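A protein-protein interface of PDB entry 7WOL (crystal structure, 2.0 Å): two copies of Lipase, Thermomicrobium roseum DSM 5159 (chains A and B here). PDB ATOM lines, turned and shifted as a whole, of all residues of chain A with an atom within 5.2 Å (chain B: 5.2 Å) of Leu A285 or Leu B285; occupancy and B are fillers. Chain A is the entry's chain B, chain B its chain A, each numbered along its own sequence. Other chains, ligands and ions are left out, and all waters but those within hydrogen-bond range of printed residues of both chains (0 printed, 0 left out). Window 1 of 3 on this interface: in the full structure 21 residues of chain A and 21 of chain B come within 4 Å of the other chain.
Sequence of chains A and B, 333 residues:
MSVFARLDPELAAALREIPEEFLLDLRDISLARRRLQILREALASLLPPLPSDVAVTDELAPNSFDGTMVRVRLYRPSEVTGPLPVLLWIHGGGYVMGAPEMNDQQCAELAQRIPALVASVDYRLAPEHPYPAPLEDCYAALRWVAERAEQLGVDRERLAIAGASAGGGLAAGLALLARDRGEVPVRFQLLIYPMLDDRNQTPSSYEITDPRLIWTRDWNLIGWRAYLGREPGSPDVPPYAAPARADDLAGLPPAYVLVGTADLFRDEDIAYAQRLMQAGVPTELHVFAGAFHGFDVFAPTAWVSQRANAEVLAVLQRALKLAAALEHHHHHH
The backbone carbonyl oxygen (O) of Val B257 sits at hydrogen-bond distance from the backbone NH (N) of His B286 (2.9 Å).
The backbone carbonyl oxygen (O) of His B286 lies within hydrogen-bond range of the backbone NH (N) of Val B259 (3.1 Å).
N of Val A257 sits at hydrogen-bond distance from O of Glu A284 (2.8 Å).
N of Val B257 lies within hydrogen-bond range of O of Glu B284 (2.8 Å).
O of Val A257 is in hydrogen-bond range of N of His A286 (2.9 Å).
N of Val A259 is in hydrogen-bond range of O of His A286 (3.1 Å).
Of the 12 printed residues of chain B, 6 touch a printed residue of chain A.
Hydrophobic or aromatic side chains of chain B that line the printed part of chain A: Ile B270, Met B277, Leu B285, His B286 and Val B287.
Hydrophobic or aromatic side chains of chain A within 4 Å of the printed part of chain B: Ile A270, Met A277, Leu A285, His A286 and Val A287.
Ile B270 touches Ile A270 (CG2 to CG2, 3.9 Å).
Ile A270 touches Met B277 (CD1 to SD, 3.8 Å).
Met A277 touches Ile B270.
Met A277 touches Val B287.
O of Val B287 touches CA of Glu A284, at 3.2 Å.
Leu A285 touches Leu B285.
CA of His B286 touches O of Leu A285 (3.3 Å).
His A286 touches Leu B285 (CA to O, 3.3 Å).
Val A287 touches Met B277.
Glu B284 touches Val A287 (CA to O, 3.2 Å).
Of chain B, only Leu B285 (3.7 Å), His B286 (3.3 Å) and Val B287 (2.8 Å) come within 4 Å of Leu A285.
Printed residues of chain B within 4 Å of Val A287: Met B277, Glu B284 and Leu B285.
Of the printed residues of chain A, Glu B284 touches His A286 and Val A287.
Leu B285 touches three residues of chain A.
Of the printed residues of chain A, His B286 touches Glu A284, Leu A285 and His A286.
The nearest printed residue of chain A that does not touch Val B287 is Thr A283 (4.2 Å).
Ile A270 touches Met B277, and with the chains exchanged Met A277 touches Ile B270.
Glu A284 touches Val B287, and with the chains exchanged Val A287 touches Glu B284.
Leu A285 touches Val B287, and with the chains exchanged Val A287 touches Leu B285.
His B286 touches its own counterpart, His A286.
A ring nitrogen (NE2) of His A286 sits at hydrogen-bond distance from the side-chain carboxylate of Glu B284 (2.7 Å).
N of Val A287 is in hydrogen-bond range of O of Leu B285, at 2.8 Å.
NE2 of His B286 lies within hydrogen-bond range of OE1 of Glu A284, 2.7 Å away.
The backbone NH of Val B287 is in hydrogen-bond range of the backbone carbonyl oxygen of Leu A285 (2.8 Å).
A ring nitrogen (ND1) of His A286 lies close to a ring nitrogen (ND1) of His B286, 3.3 Å away.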
ATOM      1  N   VAL A 257     -28.329  -5.363  12.916  1.00  0.00           N
ATOM      2  CA  VAL A 257     -28.154  -6.763  13.372  1.00  0.00           C
ATOM      3  C   VAL A 257     -27.044  -7.418  12.562  1.00  0.00           C
ATOM      4  O   VAL A 257     -27.109  -7.400  11.318  1.00  0.00           O
ATOM      5  CB  VAL A 257     -29.467  -7.545  13.246  1.00  0.00           C
ATOM      6  CG1 VAL A 257     -29.303  -8.937  13.809  1.00  0.00           C
ATOM      7  CG2 VAL A 257     -30.621  -6.811  13.908  1.00  0.00           C
ATOM      8  N   LEU A 258     -26.102  -8.013  13.275  1.00  0.00           N
ATOM      9  CA  LEU A 258     -24.965  -8.784  12.742  1.00  0.00           C
ATOM     10  C   LEU A 258     -25.076 -10.231  13.243  1.00  0.00           C
ATOM     11  O   LEU A 258     -25.322 -10.420  14.444  1.00  0.00           O
ATOM     12  CB  LEU A 258     -23.742  -8.084  13.333  1.00  0.00           C
ATOM     13  CG  LEU A 258     -22.368  -8.647  13.044  1.00  0.00           C
ATOM     14  CD1 LEU A 258     -21.331  -7.536  13.256  1.00  0.00           C
ATOM     15  CD2 LEU A 258     -22.054  -9.856  13.899  1.00  0.00           C
ATOM     16  N   VAL A 259     -24.794 -11.208  12.386  1.00  0.00           N
ATOM     17  CA  VAL A 259     -24.642 -12.629  12.790  1.00  0.00           C
ATOM     18  C   VAL A 259     -23.834 -13.373  11.729  1.00  0.00           C
ATOM     19  O   VAL A 259     -23.832 -12.937  10.559  1.00  0.00           O
ATOM     20  CB  VAL A 259     -26.021 -13.264  13.045  1.00  0.00           C
ATOM     21  CG1 VAL A 259     -26.838 -13.424  11.773  1.00  0.00           C
ATOM     22  CG2 VAL A 259     -25.888 -14.583  13.794  1.00  0.00           C
ATOM     23  N   ASP A 269     -31.904 -14.415  14.335  1.00  0.00           N
ATOM     24  CA  ASP A 269     -31.398 -13.030  14.138  1.00  0.00           C
ATOM     25  C   ASP A 269     -31.897 -12.527  12.793  1.00  0.00           C
ATOM     26  O   ASP A 269     -32.352 -11.365  12.701  1.00  0.00           O
ATOM     27  CB  ASP A 269     -29.875 -12.989  14.250  1.00  0.00           C
ATOM     28  CG  ASP A 269     -29.374 -13.234  15.663  1.00  0.00           C
ATOM     29  OD1 ASP A 269     -30.223 -13.365  16.586  1.00  0.00           O
ATOM     30  OD2 ASP A 269     -28.142 -13.281  15.840  1.00  0.00           O
ATOM     31  N   ILE A 270     -31.842 -13.381  11.773  1.00  0.00           N
ATOM     32  CA  ILE A 270     -32.382 -13.008  10.441  1.00  0.00           C
ATOM     33  C   ILE A 270     -33.879 -12.734  10.575  1.00  0.00           C
ATOM     34  O   ILE A 270     -34.337 -11.741   9.999  1.00  0.00           O
ATOM     35  CB  ILE A 270     -32.093 -14.063   9.351  1.00  0.00           C
ATOM     36  CG1 ILE A 270     -30.617 -14.135   8.983  1.00  0.00           C
ATOM     37  CG2 ILE A 270     -32.954 -13.786   8.125  1.00  0.00           C
ATOM     38  CD1 ILE A 270     -30.260 -15.361   8.172  1.00  0.00           C
ATOM     39  N   ALA A 273     -34.637  -9.325  12.431  1.00  0.00           N
ATOM     40  CA  ALA A 273     -34.281  -8.199  11.536  1.00  0.00           C
ATOM     41  C   ALA A 273     -35.340  -8.073  10.439  1.00  0.00           C
ATOM     42  O   ALA A 273     -35.807  -6.947  10.171  1.00  0.00           O
ATOM     43  CB  ALA A 273     -32.894  -8.402  10.983  1.00  0.00           C
ATOM     44  N   MET A 277     -38.065  -4.935   9.749  1.00  0.00           N
ATOM     45  CA  MET A 277     -38.208  -4.292   8.418  1.00  0.00           C
ATOM     46  C   MET A 277     -39.669  -4.315   8.021  1.00  0.00           C
ATOM     47  O   MET A 277     -40.138  -3.302   7.534  1.00  0.00           O
ATOM     48  CB  MET A 277     -37.408  -5.020   7.337  1.00  0.00           C
ATOM     49  CG  MET A 277     -35.943  -4.981   7.610  1.00  0.00           C
ATOM     50  SD  MET A 277     -35.049  -6.175   6.584  1.00  0.00           S
ATOM     51  CE  MET A 277     -33.454  -6.146   7.389  1.00  0.00           C
ATOM     52  N   THR A 283     -33.766  -0.845   9.420  1.00  0.00           N
ATOM     53  CA  THR A 283     -32.932  -1.954   9.932  1.00  0.00           C
ATOM     54  C   THR A 283     -31.908  -2.335   8.879  1.00  0.00           C
ATOM     55  O   THR A 283     -32.307  -2.532   7.706  1.00  0.00           O
ATOM     56  CB  THR A 283     -33.774  -3.189  10.298  1.00  0.00           C
ATOM     57  OG1 THR A 283     -34.726  -2.794  11.278  1.00  0.00           O
ATOM     58  CG2 THR A 283     -32.961  -4.352  10.829  1.00  0.00           C
ATOM     59  N   GLU A 284     -30.657  -2.427   9.306  1.00  0.00           N
ATOM     60  CA  GLU A 284     -29.553  -3.014   8.530  1.00  0.00           C
ATOM     61  C   GLU A 284     -29.285  -4.400   9.110  1.00  0.00           C
ATOM     62  O   GLU A 284     -29.181  -4.530  10.345  1.00  0.00           O
ATOM     63  CB  GLU A 284     -28.333  -2.100   8.585  1.00  0.00           C
ATOM     64  CG  GLU A 284     -27.106  -2.648   7.914  1.00  0.00           C
ATOM     65  CD  GLU A 284     -25.990  -1.624   7.740  1.00  0.00           C
ATOM     66  OE1 GLU A 284     -24.876  -2.050   7.396  1.00  0.00           O
ATOM     67  OE2 GLU A 284     -26.227  -0.399   7.986  1.00  0.00           O
ATOM     68  N   LEU A 285     -29.172  -5.391   8.230  1.00  0.00           N
ATOM     69  CA  LEU A 285     -28.861  -6.782   8.604  1.00  0.00           C
ATOM     70  C   LEU A 285     -27.618  -7.198   7.828  1.00  0.00           C
ATOM     71  O   LEU A 285     -27.604  -7.002   6.592  1.00  0.00           O
ATOM     72  CB  LEU A 285     -30.063  -7.663   8.256  1.00  0.00           C
ATOM     73  CG  LEU A 285     -29.790  -9.157   8.336  1.00  0.00           C
ATOM     74  CD1 LEU A 285     -29.491  -9.583   9.760  1.00  0.00           C
ATOM     75  CD2 LEU A 285     -30.961  -9.928   7.752  1.00  0.00           C
ATOM     76  N   HIS A 286     -26.599  -7.682   8.525  1.00  0.00           N
ATOM     77  CA  HIS A 286     -25.391  -8.213   7.875  1.00  0.00           C
ATOM     78  C   HIS A 286     -25.139  -9.607   8.419  1.00  0.00           C
ATOM     79  O   HIS A 286     -24.790  -9.737   9.629  1.00  0.00           O
ATOM     80  CB  HIS A 286     -24.197  -7.269   8.052  1.00  0.00           C
ATOM     81  CG  HIS A 286     -23.170  -7.404   6.977  1.00  0.00           C
ATOM     82  ND1 HIS A 286     -22.201  -6.446   6.758  1.00  0.00           N
ATOM     83  CD2 HIS A 286     -22.960  -8.383   6.065  1.00  0.00           C
ATOM     84  CE1 HIS A 286     -21.420  -6.836   5.763  1.00  0.00           C
ATOM     85  NE2 HIS A 286     -21.877  -8.023   5.307  1.00  0.00           N
ATOM     86  N   VAL A 287     -25.302 -10.605   7.546  1.00  0.00           N
ATOM     87  CA  VAL A 287     -24.912 -12.010   7.825  1.00  0.00           C
ATOM     88  C   VAL A 287     -23.565 -12.251   7.159  1.00  0.00           C
ATOM     89  O   VAL A 287     -23.471 -12.083   5.920  1.00  0.00           O
ATOM     90  CB  VAL A 287     -25.973 -13.020   7.349  1.00  0.00           C
ATOM     91  CG1 VAL A 287     -25.609 -14.433   7.801  1.00  0.00           C
ATOM     92  CG2 VAL A 287     -27.358 -12.620   7.816  1.00  0.00           C
ATOM     93  N   VAL B 257     -25.356 -11.609  -1.326  1.00  0.00           N
ATOM     94  CA  VAL B 257     -26.674 -11.015  -1.670  1.00  0.00           C
ATOM     95  C   VAL B 257     -26.772  -9.663  -0.969  1.00  0.00           C
ATOM     96  O   VAL B 257     -26.531  -9.617   0.253  1.00  0.00           O
ATOM     97  CB  VAL B 257     -27.842 -11.938  -1.296  1.00  0.00           C
ATOM     98  CG1 VAL B 257     -29.176 -11.310  -1.667  1.00  0.00           C
ATOM     99  CG2 VAL B 257     -27.690 -13.303  -1.960  1.00  0.00           C
ATOM    100  N   LEU B 258     -27.148  -8.635  -1.728  1.00  0.00           N
ATOM    101  CA  LEU B 258     -27.362  -7.253  -1.252  1.00  0.00           C
ATOM    102  C   LEU B 258     -28.762  -6.827  -1.664  1.00  0.00           C
ATOM    103  O   LEU B 258     -29.207  -7.190  -2.786  1.00  0.00           O
ATOM    104  CB  LEU B 258     -26.251  -6.451  -1.923  1.00  0.00           C
ATOM    105  CG  LEU B 258     -26.255  -4.938  -1.884  1.00  0.00           C
ATOM    106  CD1 LEU B 258     -24.872  -4.459  -2.307  1.00  0.00           C
ATOM    107  CD2 LEU B 258     -27.338  -4.327  -2.753  1.00  0.00           C
ATOM    108  N   VAL B 259     -29.469  -6.130  -0.775  1.00  0.00           N
ATOM    109  CA  VAL B 259     -30.797  -5.540  -1.088  1.00  0.00           C
ATOM    110  C   VAL B 259     -31.056  -4.406  -0.089  1.00  0.00           C
ATOM    111  O   VAL B 259     -30.542  -4.471   1.029  1.00  0.00           O
ATOM    112  CB  VAL B 259     -31.902  -6.619  -1.080  1.00  0.00           C
ATOM    113  CG1 VAL B 259     -32.160  -7.177   0.307  1.00  0.00           C
ATOM    114  CG2 VAL B 259     -33.198  -6.130  -1.704  1.00  0.00           C
ATOM    115  N   ASP B 269     -35.200 -11.739  -1.551  1.00  0.00           N
ATOM    116  CA  ASP B 269     -33.719 -11.757  -1.510  1.00  0.00           C
ATOM    117  C   ASP B 269     -33.266 -12.333  -0.167  1.00  0.00           C
ATOM    118  O   ASP B 269     -32.321 -13.142  -0.131  1.00  0.00           O
ATOM    119  CB  ASP B 269     -33.137 -10.372  -1.812  1.00  0.00           C
ATOM    120  CG  ASP B 269     -33.344  -9.910  -3.254  1.00  0.00           C
ATOM    121  OD1 ASP B 269     -33.958 -10.674  -4.044  1.00  0.00           O
ATOM    122  OD2 ASP B 269     -32.941  -8.773  -3.566  1.00  0.00           O
ATOM    123  N   ILE B 270     -33.881 -11.886   0.923  1.00  0.00           N
ATOM    124  CA  ILE B 270     -33.523 -12.387   2.275  1.00  0.00           C
ATOM    125  C   ILE B 270     -33.827 -13.891   2.302  1.00  0.00           C
ATOM    126  O   ILE B 270     -32.982 -14.643   2.750  1.00  0.00           O
ATOM    127  CB  ILE B 270     -34.279 -11.620   3.373  1.00  0.00           C
ATOM    128  CG1 ILE B 270     -33.774 -10.174   3.504  1.00  0.00           C
ATOM    129  CG2 ILE B 270     -34.184 -12.378   4.676  1.00  0.00           C
ATOM    130  CD1 ILE B 270     -34.678  -9.248   4.327  1.00  0.00           C
ATOM    131  N   ALA B 273     -31.276 -15.946   0.249  1.00  0.00           N
ATOM    132  CA  ALA B 273     -29.986 -15.950   0.987  1.00  0.00           C
ATOM    133  C   ALA B 273     -30.063 -16.916   2.183  1.00  0.00           C
ATOM    134  O   ALA B 273     -29.131 -17.699   2.411  1.00  0.00           O
ATOM    135  CB  ALA B 273     -29.620 -14.550   1.439  1.00  0.00           C
ATOM    136  N   MET B 277     -28.028 -20.489   2.976  1.00  0.00           N
ATOM    137  CA  MET B 277     -27.293 -20.757   4.237  1.00  0.00           C
ATOM    138  C   MET B 277     -27.795 -22.088   4.810  1.00  0.00           C
ATOM    139  O   MET B 277     -26.984 -22.878   5.289  1.00  0.00           O
ATOM    140  CB  MET B 277     -27.511 -19.657   5.280  1.00  0.00           C
ATOM    141  CG  MET B 277     -26.956 -18.310   4.870  1.00  0.00           C
ATOM    142  SD  MET B 277     -27.741 -17.013   5.867  1.00  0.00           S
ATOM    143  CE  MET B 277     -27.278 -15.558   4.920  1.00  0.00           C
ATOM    144  N   THR B 283     -22.692 -18.010   2.473  1.00  0.00           N
ATOM    145  CA  THR B 283     -23.512 -16.891   1.952  1.00  0.00           C
ATOM    146  C   THR B 283     -23.359 -15.694   2.883  1.00  0.00           C
ATOM    147  O   THR B 283     -23.542 -15.854   4.112  1.00  0.00           O
ATOM    148  CB  THR B 283     -24.989 -17.285   1.774  1.00  0.00           C
ATOM    149  OG1 THR B 283     -25.066 -18.412   0.901  1.00  0.00           O
ATOM    150  CG2 THR B 283     -25.847 -16.176   1.204  1.00  0.00           C
ATOM    151  N   GLU B 284     -23.014 -14.556   2.292  1.00  0.00           N
ATOM    152  CA  GLU B 284     -23.052 -13.229   2.925  1.00  0.00           C
ATOM    153  C   GLU B 284     -24.309 -12.498   2.443  1.00  0.00           C
ATOM    154  O   GLU B 284     -24.607 -12.473   1.230  1.00  0.00           O
ATOM    155  CB  GLU B 284     -21.729 -12.526   2.644  1.00  0.00           C
ATOM    156  CG  GLU B 284     -21.695 -11.135   3.241  1.00  0.00           C
ATOM    157  CD  GLU B 284     -20.396 -10.357   3.121  1.00  0.00           C
ATOM    158  OE1 GLU B 284     -19.332 -10.971   2.858  1.00  0.00           O
ATOM    159  OE2 GLU B 284     -20.461  -9.121   3.343  1.00  0.00           O
ATOM    160  N   LEU B 285     -25.097 -11.997   3.385  1.00  0.00           N
ATOM    161  CA  LEU B 285     -26.329 -11.219   3.137  1.00  0.00           C
ATOM    162  C   LEU B 285     -26.165  -9.843   3.775  1.00  0.00           C
ATOM    163  O   LEU B 285     -25.859  -9.777   4.978  1.00  0.00           O
ATOM    164  CB  LEU B 285     -27.531 -11.947   3.743  1.00  0.00           C
ATOM    165  CG  LEU B 285     -28.822 -11.134   3.763  1.00  0.00           C
ATOM    166  CD1 LEU B 285     -29.293 -10.806   2.358  1.00  0.00           C
ATOM    167  CD2 LEU B 285     -29.914 -11.873   4.517  1.00  0.00           C
ATOM    168  N   HIS B 286     -26.379  -8.785   3.006  1.00  0.00           N
ATOM    169  CA  HIS B 286     -26.342  -7.401   3.533  1.00  0.00           C
ATOM    170  C   HIS B 286     -27.604  -6.675   3.092  1.00  0.00           C
ATOM    171  O   HIS B 286     -27.804  -6.463   1.854  1.00  0.00           O
ATOM    172  CB  HIS B 286     -25.043  -6.701   3.135  1.00  0.00           C
ATOM    173  CG  HIS B 286     -24.693  -5.577   4.054  1.00  0.00           C
ATOM    174  ND1 HIS B 286     -23.427  -5.004   4.082  1.00  0.00           N
ATOM    175  CD2 HIS B 286     -25.429  -4.935   5.000  1.00  0.00           C
ATOM    176  CE1 HIS B 286     -23.400  -4.069   5.023  1.00  0.00           C
ATOM    177  NE2 HIS B 286     -24.629  -3.994   5.589  1.00  0.00           N
ATOM    178  N   VAL B 287     -28.478  -6.387   4.052  1.00  0.00           N
ATOM    179  CA  VAL B 287     -29.698  -5.574   3.812  1.00  0.00           C
ATOM    180  C   VAL B 287     -29.392  -4.159   4.310  1.00  0.00           C
ATOM    181  O   VAL B 287     -29.005  -4.020   5.506  1.00  0.00           O
ATOM    182  CB  VAL B 287     -30.956  -6.153   4.478  1.00  0.00           C
ATOM    183  CG1 VAL B 287     -32.200  -5.358   4.083  1.00  0.00           C
ATOM    184  CG2 VAL B 287     -31.118  -7.624   4.173  1.00  0.00           C
